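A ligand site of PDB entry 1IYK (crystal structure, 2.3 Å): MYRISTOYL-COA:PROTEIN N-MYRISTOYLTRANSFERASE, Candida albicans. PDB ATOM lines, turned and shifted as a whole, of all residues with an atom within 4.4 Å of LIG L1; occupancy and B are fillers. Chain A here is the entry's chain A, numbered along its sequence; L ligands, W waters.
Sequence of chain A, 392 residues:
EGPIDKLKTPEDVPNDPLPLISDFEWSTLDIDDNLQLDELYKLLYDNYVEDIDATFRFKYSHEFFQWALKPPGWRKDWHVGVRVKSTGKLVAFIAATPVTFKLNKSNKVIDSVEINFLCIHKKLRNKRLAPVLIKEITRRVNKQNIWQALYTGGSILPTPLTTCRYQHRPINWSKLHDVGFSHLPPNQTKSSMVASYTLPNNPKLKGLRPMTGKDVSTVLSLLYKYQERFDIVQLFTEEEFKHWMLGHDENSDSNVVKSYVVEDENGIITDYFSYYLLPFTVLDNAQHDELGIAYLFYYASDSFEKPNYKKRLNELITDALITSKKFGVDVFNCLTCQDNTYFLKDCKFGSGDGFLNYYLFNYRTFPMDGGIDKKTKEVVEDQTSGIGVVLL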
ATOM      1  N   VAL A  49      19.181   2.401   1.210  1.00  0.00           N
ATOM      2  CA  VAL A  49      20.359   2.608   0.358  1.00  0.00           C
ATOM      3  C   VAL A  49      20.475   1.695  -0.855  1.00  0.00           C
ATOM      4  O   VAL A  49      20.353   0.471  -0.767  1.00  0.00           O
ATOM      5  CB  VAL A  49      21.655   2.499   1.203  1.00  0.00           C
ATOM      6  CG1 VAL A  49      22.857   2.760   0.326  1.00  0.00           C
ATOM      7  CG2 VAL A  49      21.620   3.484   2.351  1.00  0.00           C
ATOM      8  N   GLU A  50      20.736   2.327  -1.988  1.00  0.00           N
ATOM      9  CA  GLU A  50      20.903   1.662  -3.279  1.00  0.00           C
ATOM     10  C   GLU A  50      22.271   2.034  -3.825  1.00  0.00           C
ATOM     11  O   GLU A  50      22.887   2.996  -3.348  1.00  0.00           O
ATOM     12  CB  GLU A  50      19.817   2.143  -4.256  1.00  0.00           C
ATOM     13  CG  GLU A  50      18.433   1.572  -3.992  1.00  0.00           C
ATOM     14  CD  GLU A  50      17.336   2.318  -4.744  1.00  0.00           C
ATOM     15  OE1 GLU A  50      17.623   2.913  -5.808  1.00  0.00           O
ATOM     16  OE2 GLU A  50      16.173   2.296  -4.273  1.00  0.00           O
ATOM     17  N   ASP A  51      22.744   1.280  -4.812  1.00  0.00           N
ATOM     18  CA  ASP A  51      24.030   1.604  -5.434  1.00  0.00           C
ATOM     19  C   ASP A  51      23.757   2.773  -6.393  1.00  0.00           C
ATOM     20  O   ASP A  51      22.605   3.096  -6.682  1.00  0.00           O
ATOM     21  CB  ASP A  51      24.551   0.410  -6.232  1.00  0.00           C
ATOM     22  CG  ASP A  51      23.698   0.099  -7.445  1.00  0.00           C
ATOM     23  OD1 ASP A  51      24.232   0.182  -8.581  1.00  0.00           O
ATOM     24  OD2 ASP A  51      22.494  -0.207  -7.265  1.00  0.00           O
ATOM     25  N   ASP A  53      23.698   3.086  -9.512  1.00  0.00           N
ATOM     26  CA  ASP A  53      22.866   2.794 -10.687  1.00  0.00           C
ATOM     27  C   ASP A  53      21.472   2.246 -10.403  1.00  0.00           C
ATOM     28  O   ASP A  53      20.774   1.835 -11.323  1.00  0.00           O
ATOM     29  CB  ASP A  53      23.597   1.828 -11.607  1.00  0.00           C
ATOM     30  CG  ASP A  53      24.823   2.442 -12.261  1.00  0.00           C
ATOM     31  OD1 ASP A  53      25.749   1.695 -12.605  1.00  0.00           O
ATOM     32  OD2 ASP A  53      24.858   3.679 -12.444  1.00  0.00           O
ATOM     33  N   PHE A  56      20.787  -2.435  -7.143  1.00  0.00           N
ATOM     34  CA  PHE A  56      20.693  -3.186  -5.888  1.00  0.00           C
ATOM     35  C   PHE A  56      20.326  -2.317  -4.693  1.00  0.00           C
ATOM     36  O   PHE A  56      20.566  -1.105  -4.688  1.00  0.00           O
ATOM     37  CB  PHE A  56      22.046  -3.832  -5.583  1.00  0.00           C
ATOM     38  CG  PHE A  56      22.630  -4.602  -6.737  1.00  0.00           C
ATOM     39  CD1 PHE A  56      22.131  -5.863  -7.073  1.00  0.00           C
ATOM     40  CD2 PHE A  56      23.685  -4.078  -7.476  1.00  0.00           C
ATOM     41  CE1 PHE A  56      22.688  -6.592  -8.144  1.00  0.00           C
ATOM     42  CE2 PHE A  56      24.250  -4.793  -8.553  1.00  0.00           C
ATOM     43  CZ  PHE A  56      23.753  -6.059  -8.879  1.00  0.00           C
ATOM     44  N   PHE A  58      20.274  -2.468  -0.206  1.00  0.00           N
ATOM     45  CA  PHE A  58      20.587  -3.185   1.026  1.00  0.00           C
ATOM     46  C   PHE A  58      19.315  -3.850   1.534  1.00  0.00           C
ATOM     47  O   PHE A  58      18.219  -3.298   1.406  1.00  0.00           O
ATOM     48  CB  PHE A  58      21.120  -2.205   2.100  1.00  0.00           C
ATOM     49  CG  PHE A  58      22.586  -1.870   1.952  1.00  0.00           C
ATOM     50  CD1 PHE A  58      23.556  -2.666   2.544  1.00  0.00           C
ATOM     51  CD2 PHE A  58      22.994  -0.764   1.209  1.00  0.00           C
ATOM     52  CE1 PHE A  58      24.924  -2.363   2.414  1.00  0.00           C
ATOM     53  CE2 PHE A  58      24.362  -0.448   1.073  1.00  0.00           C
ATOM     54  CZ  PHE A  58      25.322  -1.248   1.676  1.00  0.00           C
ATOM     55  N   TYR A  60      18.214  -5.507   5.033  1.00  0.00           N
ATOM     56  CA  TYR A  60      18.415  -5.840   6.426  1.00  0.00           C
ATOM     57  C   TYR A  60      17.240  -6.693   6.873  1.00  0.00           C
ATOM     58  O   TYR A  60      16.090  -6.302   6.686  1.00  0.00           O
ATOM     59  CB  TYR A  60      18.482  -4.555   7.262  1.00  0.00           C
ATOM     60  CG  TYR A  60      19.771  -3.773   7.112  1.00  0.00           C
ATOM     61  CD1 TYR A  60      20.864  -4.042   7.935  1.00  0.00           C
ATOM     62  CD2 TYR A  60      19.910  -2.770   6.148  1.00  0.00           C
ATOM     63  CE1 TYR A  60      22.069  -3.339   7.815  1.00  0.00           C
ATOM     64  CE2 TYR A  60      21.113  -2.060   6.009  1.00  0.00           C
ATOM     65  CZ  TYR A  60      22.178  -2.338   6.852  1.00  0.00           C
ATOM     66  OH  TYR A  60      23.354  -1.617   6.763  1.00  0.00           O
ATOM     67  N   ASN A 116      22.653   5.366  12.616  1.00  0.00           N
ATOM     68  CA  ASN A 116      22.499   4.507  11.459  1.00  0.00           C
ATOM     69  C   ASN A 116      21.024   4.409  11.065  1.00  0.00           C
ATOM     70  O   ASN A 116      20.157   4.913  11.783  1.00  0.00           O
ATOM     71  CB  ASN A 116      23.077   3.132  11.825  1.00  0.00           C
ATOM     72  CG  ASN A 116      23.303   2.231  10.618  1.00  0.00           C
ATOM     73  OD1 ASN A 116      23.214   2.654   9.467  1.00  0.00           O
ATOM     74  ND2 ASN A 116      23.617   0.970  10.891  1.00  0.00           N
ATOM     75  N   THR A 152      28.779   6.893   9.410  1.00  0.00           N
ATOM     76  CA  THR A 152      29.349   6.837   8.086  1.00  0.00           C
ATOM     77  C   THR A 152      28.310   7.375   7.106  1.00  0.00           C
ATOM     78  O   THR A 152      27.150   7.518   7.459  1.00  0.00           O
ATOM     79  CB  THR A 152      29.701   5.392   7.689  1.00  0.00           C
ATOM     80  OG1 THR A 152      28.514   4.590   7.681  1.00  0.00           O
ATOM     81  CG2 THR A 152      30.695   4.790   8.690  1.00  0.00           C
ATOM     82  N   GLY A 153      28.746   7.669   5.889  1.00  0.00           N
ATOM     83  CA  GLY A 153      27.838   8.187   4.890  1.00  0.00           C
ATOM     84  C   GLY A 153      28.529   8.448   3.562  1.00  0.00           C
ATOM     85  O   GLY A 153      29.692   8.103   3.366  1.00  0.00           O
ATOM     86  N   GLY A 154      27.790   9.069   2.643  1.00  0.00           N
ATOM     87  CA  GLY A 154      28.339   9.391   1.341  1.00  0.00           C
ATOM     88  C   GLY A 154      29.111  10.685   1.428  1.00  0.00           C
ATOM     89  O   GLY A 154      29.214  11.290   2.488  1.00  0.00           O
ATOM     90  N   TYR A 166      35.326   0.455  -1.016  1.00  0.00           N
ATOM     91  CA  TYR A 166      34.812  -0.910  -0.905  1.00  0.00           C
ATOM     92  C   TYR A 166      35.619  -1.807  -1.828  1.00  0.00           C
ATOM     93  O   TYR A 166      36.088  -1.381  -2.887  1.00  0.00           O
ATOM     94  CB  TYR A 166      33.327  -0.990  -1.291  1.00  0.00           C
ATOM     95  CG  TYR A 166      32.367  -0.546  -0.190  1.00  0.00           C
ATOM     96  CD1 TYR A 166      31.922  -1.460   0.772  1.00  0.00           C
ATOM     97  CD2 TYR A 166      31.953   0.780  -0.093  1.00  0.00           C
ATOM     98  CE1 TYR A 166      31.080  -1.047   1.797  1.00  0.00           C
ATOM     99  CE2 TYR A 166      31.122   1.200   0.945  1.00  0.00           C
ATOM    100  CZ  TYR A 166      30.685   0.284   1.883  1.00  0.00           C
ATOM    101  OH  TYR A 166      29.885   0.693   2.925  1.00  0.00           O
ATOM    102  N   HIS A 168      35.659  -6.011  -3.384  1.00  0.00           N
ATOM    103  CA  HIS A 168      34.800  -7.166  -3.613  1.00  0.00           C
ATOM    104  C   HIS A 168      35.569  -8.407  -4.053  1.00  0.00           C
ATOM    105  O   HIS A 168      36.409  -8.330  -4.960  1.00  0.00           O
ATOM    106  CB  HIS A 168      33.766  -6.816  -4.689  1.00  0.00           C
ATOM    107  CG  HIS A 168      32.979  -5.582  -4.391  1.00  0.00           C
ATOM    108  ND1 HIS A 168      32.005  -5.537  -3.425  1.00  0.00           N
ATOM    109  CD2 HIS A 168      33.030  -4.334  -4.927  1.00  0.00           C
ATOM    110  CE1 HIS A 168      31.484  -4.326  -3.375  1.00  0.00           C
ATOM    111  NE2 HIS A 168      32.094  -3.580  -4.277  1.00  0.00           N
ATOM    112  N   PRO A 170      34.659 -11.998  -5.445  1.00  0.00           N
ATOM    113  CA  PRO A 170      33.657 -12.931  -5.974  1.00  0.00           C
ATOM    114  C   PRO A 170      33.833 -14.378  -5.515  1.00  0.00           C
ATOM    115  O   PRO A 170      34.940 -14.922  -5.514  1.00  0.00           O
ATOM    116  CB  PRO A 170      33.843 -12.817  -7.488  1.00  0.00           C
ATOM    117  CG  PRO A 170      34.280 -11.399  -7.657  1.00  0.00           C
ATOM    118  CD  PRO A 170      35.286 -11.230  -6.535  1.00  0.00           C
ATOM    119  N   GLY A 180      24.578  -8.274 -13.226  1.00  0.00           N
ATOM    120  CA  GLY A 180      25.206  -6.998 -13.510  1.00  0.00           C
ATOM    121  C   GLY A 180      26.068  -6.433 -12.392  1.00  0.00           C
ATOM    122  O   GLY A 180      26.387  -5.244 -12.404  1.00  0.00           O
ATOM    123  N   PHE A 181      26.441  -7.268 -11.428  1.00  0.00           N
ATOM    124  CA  PHE A 181      27.296  -6.801 -10.337  1.00  0.00           C
ATOM    125  C   PHE A 181      28.732  -6.687 -10.851  1.00  0.00           C
ATOM    126  O   PHE A 181      29.491  -5.819 -10.424  1.00  0.00           O
ATOM    127  CB  PHE A 181      27.220  -7.768  -9.159  1.00  0.00           C
ATOM    128  CG  PHE A 181      27.934  -7.292  -7.912  1.00  0.00           C
ATOM    129  CD1 PHE A 181      29.288  -7.570  -7.721  1.00  0.00           C
ATOM    130  CD2 PHE A 181      27.244  -6.601  -6.920  1.00  0.00           C
ATOM    131  CE1 PHE A 181      29.941  -7.150  -6.555  1.00  0.00           C
ATOM    132  CE2 PHE A 181      27.888  -6.176  -5.741  1.00  0.00           C
ATOM    133  CZ  PHE A 181      29.241  -6.460  -5.563  1.00  0.00           C
ATOM    134  N   SER A 182      29.108  -7.581 -11.766  1.00  0.00           N
ATOM    135  CA  SER A 182      30.445  -7.574 -12.345  1.00  0.00           C
ATOM    136  C   SER A 182      30.348  -7.753 -13.853  1.00  0.00           C
ATOM    137  O   SER A 182      29.388  -8.352 -14.350  1.00  0.00           O
ATOM    138  CB  SER A 182      31.284  -8.707 -11.755  1.00  0.00           C
ATOM    139  OG  SER A 182      30.779  -9.963 -12.185  1.00  0.00           O
ATOM    140  N   TYR A 197      38.471 -17.603  -9.895  1.00  0.00           N
ATOM    141  CA  TYR A 197      37.967 -17.302  -8.556  1.00  0.00           C
ATOM    142  C   TYR A 197      37.675 -18.530  -7.688  1.00  0.00           C
ATOM    143  O   TYR A 197      37.423 -18.391  -6.489  1.00  0.00           O
ATOM    144  CB  TYR A 197      36.723 -16.420  -8.659  1.00  0.00           C
ATOM    145  CG  TYR A 197      37.037 -14.990  -9.006  1.00  0.00           C
ATOM    146  CD1 TYR A 197      37.857 -14.224  -8.182  1.00  0.00           C
ATOM    147  CD2 TYR A 197      36.545 -14.401 -10.175  1.00  0.00           C
ATOM    148  CE1 TYR A 197      38.171 -12.916  -8.492  1.00  0.00           C
ATOM    149  CE2 TYR A 197      36.867 -13.089 -10.495  1.00  0.00           C
ATOM    150  CZ  TYR A 197      37.681 -12.344  -9.646  1.00  0.00           C
ATOM    151  OH  TYR A 197      37.996 -11.044  -9.937  1.00  0.00           O
ATOM    152  N   PHE A 280      21.983  -8.122  -0.735  1.00  0.00           N
ATOM    153  CA  PHE A 280      21.541  -7.076  -1.642  1.00  0.00           C
ATOM    154  C   PHE A 280      20.265  -7.602  -2.298  1.00  0.00           C
ATOM    155  O   PHE A 280      20.199  -8.772  -2.690  1.00  0.00           O
ATOM    156  CB  PHE A 280      22.560  -6.872  -2.773  1.00  0.00           C
ATOM    157  CG  PHE A 280      23.374  -5.595  -2.664  1.00  0.00           C
ATOM    158  CD1 PHE A 280      24.383  -5.351  -3.596  1.00  0.00           C
ATOM    159  CD2 PHE A 280      23.153  -4.670  -1.653  1.00  0.00           C
ATOM    160  CE1 PHE A 280      25.163  -4.196  -3.510  1.00  0.00           C
ATOM    161  CE2 PHE A 280      23.924  -3.518  -1.558  1.00  0.00           C
ATOM    162  CZ  PHE A 280      24.933  -3.284  -2.493  1.00  0.00           C
ATOM    163  N   GLY A 350      38.692  -7.060  -5.576  1.00  0.00           N
ATOM    164  CA  GLY A 350      38.736  -6.037  -6.600  1.00  0.00           C
ATOM    165  C   GLY A 350      38.104  -4.772  -6.044  1.00  0.00           C
ATOM    166  O   GLY A 350      37.295  -4.845  -5.117  1.00  0.00           O
ATOM    167  N   SER A 351      38.482  -3.609  -6.579  1.00  0.00           N
ATOM    168  CA  SER A 351      37.934  -2.338  -6.114  1.00  0.00           C
ATOM    169  C   SER A 351      36.512  -2.133  -6.642  1.00  0.00           C
ATOM    170  O   SER A 351      36.218  -2.473  -7.786  1.00  0.00           O
ATOM    171  CB  SER A 351      38.819  -1.180  -6.566  1.00  0.00           C
ATOM    172  OG  SER A 351      40.020  -1.137  -5.813  1.00  0.00           O
ATOM    173  N   GLY A 352      35.631  -1.602  -5.804  1.00  0.00           N
ATOM    174  CA  GLY A 352      34.274  -1.368  -6.239  1.00  0.00           C
ATOM    175  C   GLY A 352      34.102   0.091  -6.618  1.00  0.00           C
ATOM    176  O   GLY A 352      35.056   0.863  -6.527  1.00  0.00           O
ATOM    177  N   ASP A 353      32.908   0.468  -7.044  1.00  0.00           N
ATOM    178  CA  ASP A 353      32.661   1.855  -7.412  1.00  0.00           C
ATOM    179  C   ASP A 353      32.156   2.678  -6.223  1.00  0.00           C
ATOM    180  O   ASP A 353      31.847   3.852  -6.357  1.00  0.00           O
ATOM    181  CB  ASP A 353      31.667   1.930  -8.579  1.00  0.00           C
ATOM    182  CG  ASP A 353      30.310   1.321  -8.246  1.00  0.00           C
ATOM    183  OD1 ASP A 353      30.133   0.769  -7.144  1.00  0.00           O
ATOM    184  OD2 ASP A 353      29.397   1.402  -9.094  1.00  0.00           O
ATOM    185  N   GLY A 354      32.089   2.073  -5.032  1.00  0.00           N
ATOM    186  CA  GLY A 354      31.608   2.804  -3.880  1.00  0.00           C
ATOM    187  C   GLY A 354      32.655   3.193  -2.848  1.00  0.00           C
ATOM    188  O   GLY A 354      33.651   2.500  -2.671  1.00  0.00           O
ATOM    189  N   LEU A 356      33.250   5.091   1.280  1.00  0.00           N
ATOM    190  CA  LEU A 356      32.609   5.289   2.569  1.00  0.00           C
ATOM    191  C   LEU A 356      33.394   6.304   3.386  1.00  0.00           C
ATOM    192  O   LEU A 356      34.601   6.157   3.588  1.00  0.00           O
ATOM    193  CB  LEU A 356      32.537   3.964   3.347  1.00  0.00           C
ATOM    194  CG  LEU A 356      31.738   3.974   4.661  1.00  0.00           C
ATOM    195  CD1 LEU A 356      30.260   4.188   4.348  1.00  0.00           C
ATOM    196  CD2 LEU A 356      31.937   2.671   5.435  1.00  0.00           C
ATOM    197  N   LEU A 392      27.771  -1.150  10.917  1.00  0.00           N
ATOM    198  CA  LEU A 392      26.831  -1.992  10.192  1.00  0.00           C
ATOM    199  C   LEU A 392      26.016  -1.310   9.088  1.00  0.00           C
ATOM    200  O   LEU A 392      26.036  -0.067   8.995  1.00  0.00           O
ATOM    201  CB  LEU A 392      25.880  -2.648  11.193  1.00  0.00           C
ATOM    202  CG  LEU A 392      26.562  -3.373  12.367  1.00  0.00           C
ATOM    203  CD1 LEU A 392      25.493  -3.966  13.306  1.00  0.00           C
ATOM    204  CD2 LEU A 392      27.475  -4.461  11.825  1.00  0.00           C
ATOM    205  OXT LEU A 392      25.358  -2.042   8.328  1.00  0.00           O
HETATM  206  C1  LIG L   1      26.697   0.396   4.426  1.00  0.00           C
HETATM  207  N1  LIG L   1      25.898   1.069   6.672  1.00  0.00           N
HETATM  208  C2  LIG L   1      26.334   1.378   5.472  1.00  0.00           C
HETATM  209  N2  LIG L   1      26.392   2.749   5.307  1.00  0.00           N
HETATM  210  C3  LIG L   1      25.964   3.307   6.493  1.00  0.00           C
HETATM  211  C4  LIG L   1      25.687   2.240   7.283  1.00  0.00           C
HETATM  212  C5  LIG L   1      26.799   3.605   4.164  1.00  0.00           C
HETATM  213  C6  LIG L   1      25.576   4.114   3.405  1.00  0.00           C
HETATM  214  C7  LIG L   1      25.950   5.305   2.527  1.00  0.00           C
HETATM  215  C8  LIG L   1      27.106   5.055   1.549  1.00  0.00           C
HETATM  216  C9  LIG L   1      26.886   3.884   0.631  1.00  0.00           C
HETATM  217  C10 LIG L   1      27.585   2.697   0.888  1.00  0.00           C
HETATM  218  C11 LIG L   1      27.397   1.598   0.060  1.00  0.00           C
HETATM  219  C12 LIG L   1      26.518   1.673  -1.041  1.00  0.00           C
HETATM  220  C13 LIG L   1      25.817   2.873  -1.303  1.00  0.00           C
HETATM  221  C14 LIG L   1      26.006   3.978  -0.463  1.00  0.00           C
HETATM  222  C15 LIG L   1      26.330   0.468  -1.953  1.00  0.00           C
HETATM  223  C16 LIG L   1      27.364   0.432  -3.073  1.00  0.00           C
HETATM  224  O1  LIG L   1      27.397   1.306  -3.939  1.00  0.00           O
HETATM  225  N3  LIG L   1      28.197  -0.565  -3.066  1.00  0.00           N
HETATM  226  C17 LIG L   1      29.214  -0.667  -4.048  1.00  0.00           C
HETATM  227  C18 LIG L   1      29.064  -1.912  -4.883  1.00  0.00           C
HETATM  228  O2  LIG L   1      28.554  -2.910  -4.369  1.00  0.00           O
HETATM  229  C19 LIG L   1      30.564  -0.645  -3.339  1.00  0.00           C
HETATM  230  O3  LIG L   1      31.590  -0.855  -4.267  1.00  0.00           O
HETATM  231  N4  LIG L   1      29.471  -1.852  -6.136  1.00  0.00           N
HETATM  232  C20 LIG L   1      29.426  -3.024  -6.983  1.00  0.00           C
HETATM  233  C21 LIG L   1      30.742  -3.128  -7.691  1.00  0.00           C
HETATM  234  O4  LIG L   1      31.507  -2.156  -7.687  1.00  0.00           O
HETATM  235  C22 LIG L   1      28.205  -3.098  -7.930  1.00  0.00           C
HETATM  236  C23 LIG L   1      28.119  -1.906  -8.929  1.00  0.00           C
HETATM  237  C24 LIG L   1      26.886  -2.072  -9.835  1.00  0.00           C
HETATM  238  C25 LIG L   1      26.666  -0.823 -10.692  1.00  0.00           C
HETATM  239  N5  LIG L   1      26.555   0.321  -9.788  1.00  0.00           N
HETATM  240  N6  LIG L   1      30.981  -4.251  -8.285  1.00  0.00           N
HETATM  241  C26 LIG L   1      32.216  -4.533  -9.012  1.00  0.00           C
HETATM  242  C27 LIG L   1      32.602  -5.991  -8.727  1.00  0.00           C
HETATM  243  C28 LIG L   1      33.964  -6.407  -9.324  1.00  0.00           C
HETATM  244  C29 LIG L   1      35.131  -5.475  -8.887  1.00  0.00           C
HETATM  245  C30 LIG L   1      36.486  -5.969  -9.504  1.00  0.00           C
HETATM  246  C31 LIG L   1      36.799  -7.427  -9.115  1.00  0.00           C
HETATM  247  C32 LIG L   1      35.641  -8.349  -9.549  1.00  0.00           C
HETATM  248  C33 LIG L   1      34.297  -7.873  -8.940  1.00  0.00           C
HETATM  249  S1  LG2 L   2      23.895   6.968   6.127  1.00  0.00           S
HETATM  250  C1  LG2 L   2      22.462   6.194   5.300  1.00  0.00           C
HETATM  251  C2  LG2 L   2      21.519   7.294   4.782  1.00  0.00           C
HETATM  252  N1  LG2 L   2      20.276   6.730   4.280  1.00  0.00           N
HETATM  253  C3  LG2 L   2      20.030   6.621   3.018  1.00  0.00           C
HETATM  254  O1  LG2 L   2      20.803   6.977   2.109  1.00  0.00           O
HETATM  255  C4  LG2 L   2      18.696   6.001   2.622  1.00  0.00           C
HETATM  256  C5  LG2 L   2      18.175   6.502   1.237  1.00  0.00           C
HETATM  257  N2  LG2 L   2      17.978   7.970   1.240  1.00  0.00           N
HETATM  258  C6  LG2 L   2      17.095   8.492   2.043  1.00  0.00           C
HETATM  259  O2  LG2 L   2      16.327   7.837   2.758  1.00  0.00           O
HETATM  260  C7  LG2 L   2      17.027  10.012   2.088  1.00  0.00           C
HETATM  261  O3  LG2 L   2      17.610  10.567   0.907  1.00  0.00           O
HETATM  262  C8  LG2 L   2      17.693  10.643   3.347  1.00  0.00           C
HETATM  263  C9  LG2 L   2      17.718  12.168   3.116  1.00  0.00           C
HETATM  264  C10 LG2 L   2      19.160  10.260   3.487  1.00  0.00           C
HETATM  265  C11 LG2 L   2      16.939  10.236   4.655  1.00  0.00           C
HETATM  266  N3  LG2 L   2      23.672  12.113   6.032  1.00  0.00           N
HETATM  267  O4  LG2 L   2      15.005  15.628   3.795  1.00  0.00           O
HETATM  268  P1  LG2 L   2      15.960  16.253   2.847  1.00  0.00           P
HETATM  269  C12 LG2 L   2      20.915  16.265   4.809  1.00  0.00           C
HETATM  270  C13 LG2 L   2      23.533  13.298   6.696  1.00  0.00           C
HETATM  271  O5  LG2 L   2      15.300  17.258   1.943  1.00  0.00           O
HETATM  272  P2  LG2 L   2      16.056  13.655   1.617  1.00  0.00           P
HETATM  273  C14 LG2 L   2      23.197   6.947   7.744  1.00  0.00           C
HETATM  274  O6  LG2 L   2      22.147   6.324   8.001  1.00  0.00           O
HETATM  275  C15 LG2 L   2      21.734  17.282   3.974  1.00  0.00           C
HETATM  276  O7  LG2 L   2      22.274  18.264   4.853  1.00  0.00           O
HETATM  277  N4  LG2 L   2      22.822  14.342   6.287  1.00  0.00           N
HETATM  278  O8  LG2 L   2      16.755  15.102   1.965  1.00  0.00           O
HETATM  279  C16 LG2 L   2      23.886   7.705   8.846  1.00  0.00           C
HETATM  280  C17 LG2 L   2      20.730  17.962   3.047  1.00  0.00           C
HETATM  281  O9  LG2 L   2      20.541  19.294   3.525  1.00  0.00           O
HETATM  282  P3  LG2 L   2      21.480  20.486   2.856  1.00  0.00           P
HETATM  283  C18 LG2 L   2      22.160  14.108   5.141  1.00  0.00           C
HETATM  284  O10 LG2 L   2      14.595  13.823   1.532  1.00  0.00           O
HETATM  285  C19 LG2 L   2      23.261   9.134   8.883  1.00  0.00           C
HETATM  286  C20 LG2 L   2      19.479  17.106   3.250  1.00  0.00           C
HETATM  287  O11 LG2 L   2      19.539  16.480   4.530  1.00  0.00           O
HETATM  288  C21 LG2 L   2      22.222  12.866   4.343  1.00  0.00           C
HETATM  289  O12 LG2 L   2      16.664  13.069   0.383  1.00  0.00           O
HETATM  290  C22 LG2 L   2      23.949  10.093   9.860  1.00  0.00           C
HETATM  291  C23 LG2 L   2      18.145  17.772   2.952  1.00  0.00           C
HETATM  292  O13 LG2 L   2      17.140  17.041   3.647  1.00  0.00           O
HETATM  293  C24 LG2 L   2      23.096  11.899   4.844  1.00  0.00           C
HETATM  294  N5  LG2 L   2      23.348  10.743   4.117  1.00  0.00           N
HETATM  295  O14 LG2 L   2      16.388  12.707   2.918  1.00  0.00           O
HETATM  296  C25 LG2 L   2      23.170  11.451   9.925  1.00  0.00           C
HETATM  297  N6  LG2 L   2      21.404  12.941   3.247  1.00  0.00           N
HETATM  298  O15 LG2 L   2      22.760  19.813   2.304  1.00  0.00           O
HETATM  299  C26 LG2 L   2      23.902  12.532  10.763  1.00  0.00           C
HETATM  300  C27 LG2 L   2      20.884  14.158   3.310  1.00  0.00           C
HETATM  301  O16 LG2 L   2      20.620  21.092   1.747  1.00  0.00           O
HETATM  302  C28 LG2 L   2      24.161  12.138  12.235  1.00  0.00           C
HETATM  303  N7  LG2 L   2      21.292  14.913   4.425  1.00  0.00           N
HETATM  304  O17 LG2 L   2      21.785  21.482   3.978  1.00  0.00           O
HETATM  305  C29 LG2 L   2      24.903  13.292  12.970  1.00  0.00           C
HETATM  306  C30 LG2 L   2      25.075  13.037  14.462  1.00  0.00           C
HETATM  307  C31 LG2 L   2      23.715  13.089  15.217  1.00  0.00           C
HETATM  308  C32 LG2 L   2      23.848  12.603  16.664  1.00  0.00           C
HETATM  309  C33 LG2 L   2      24.664  13.548  17.581  1.00  0.00           C
HETATM  310  C34 LG2 L   2      24.750  12.948  18.987  1.00  0.00           C
HETATM  311  C35 LG2 L   2      25.747  13.725  19.907  1.00  0.00           C
HETATM  312  O   HOH W   1      22.997   1.130   7.190  1.00  0.00           O
HETATM  313  O   HOH W   2      29.553  -1.179   4.922  1.00  0.00           O
HETATM  314  O   HOH W   3      28.576  -2.104  -0.493  1.00  0.00           O
HETATM  315  O   HOH W   4      27.582   2.120  -6.536  1.00  0.00           O
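A nitrogen (N6) of LIG L1 sits at hydrogen-bond distance from the backbone carbonyl oxygen of Phe 181. The chain-end carboxylate (O) of Leu 392 sits at hydrogen-bond distance from a nitrogen (N1) of LIG L1 (2.6 Å). N5 of LIG L1 is in salt-bridge range of OD2 of Asp 353 (3.1 Å). The side-chain carboxylate of Asp 51 is in salt-bridge range of a nitrogen (N5) of LIG L1, 2.6 Å away. N of Gly 354 sits at hydrogen-bond distance from O3 of LIG L1, at 3.1 Å. The side-chain carboxylate (OD1) of Asp 53 lies within salt-bridge range of a nitrogen (N5) of LIG L1, at 3.2 Å. NE2 of His 168 sits at hydrogen-bond distance from O3 of LIG L1, 2.8 Å away. The backbone NH of Asp 353 lies within hydrogen-bond range of an oxygen (O4) of LIG L1 (3.0 Å).
The backbone NH (N) of Tyr 166 sits at hydrogen-bond distance from the backbone carbonyl oxygen (O) of Gly 354 (3.1 Å). The chain-end carboxylate of Leu 392 sits at hydrogen-bond distance from the side-chain amide nitrogen of Asn 116 (3.2 Å). The backbone NH (N) of His 168 sits at hydrogen-bond distance from the backbone carbonyl oxygen (O) of Gly 350 (2.7 Å). The chain-end carboxylate (OXT) of Leu 392 lies within hydrogen-bond range of the side-chain hydroxyl (OH) of Tyr 60, 2.6 Å away. N of Phe 56 sits at hydrogen-bond distance from OD2 of Asp 51 (2.8 Å). The backbone carbonyl oxygen (O) of Tyr 166 is in hydrogen-bond range of the backbone NH (N) of Gly 352 (3.0 Å). The side-chain carboxylate (OD1) of Asp 51 sits at hydrogen-bond distance from the backbone NH (N) of Asp 53, 3.1 Å away. The backbone NH (N) of Phe 58 sits at hydrogen-bond distance from the backbone carbonyl oxygen (O) of Val 49 (3.0 Å).
Residues that only touch LIG L1: Thr 152 (3.1 Å), Gly 352 (3.2 Å), Asn 116 (3.3 Å), Ser 351 (3.4 Å), Val 49 (3.4 Å), Tyr 166 (3.4 Å), Gly 350 (3.5 Å), Phe 58 (3.5 Å), Leu 356 (3.5 Å), Glu 50 (3.6 Å), Tyr 197 (3.6 Å), Tyr 60 (3.7 Å), Phe 280 (3.7 Å), Pro 170 (3.8 Å) and Phe 56 (3.999 Å). Hydrophobic or aromatic side chains within 4 Å of LIG L1: Val 49, Phe 56, Phe 58, Tyr 166, His 168, Pro 170, Phe 181, Phe 280 and Leu 356. 22 residues have an atom within 4 Å of LIG L1: Val 49, Glu 50, Asp 51, Asp 53, Phe 56, Phe 58, Tyr 60, Asn 116, Thr 152, Tyr 166, His 168, Pro 170, Phe 181, Tyr 197, Phe 280, Gly 350, Ser 351, Gly 352, Asp 353, Gly 354, Leu 356 and Leu 392.
Water W4 bridges O1 of LIG L1 (2.7 Å) and OD1 of Asp 353 (2.9 Å). Water W1 lies within hydrogen-bond range of the side-chain amide oxygen of Asn 116 (2.7 Å), the side-chain hydroxyl of Tyr 60 (2.8 Å) and a nitrogen (N1) of LIG L1 (2.9 Å).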
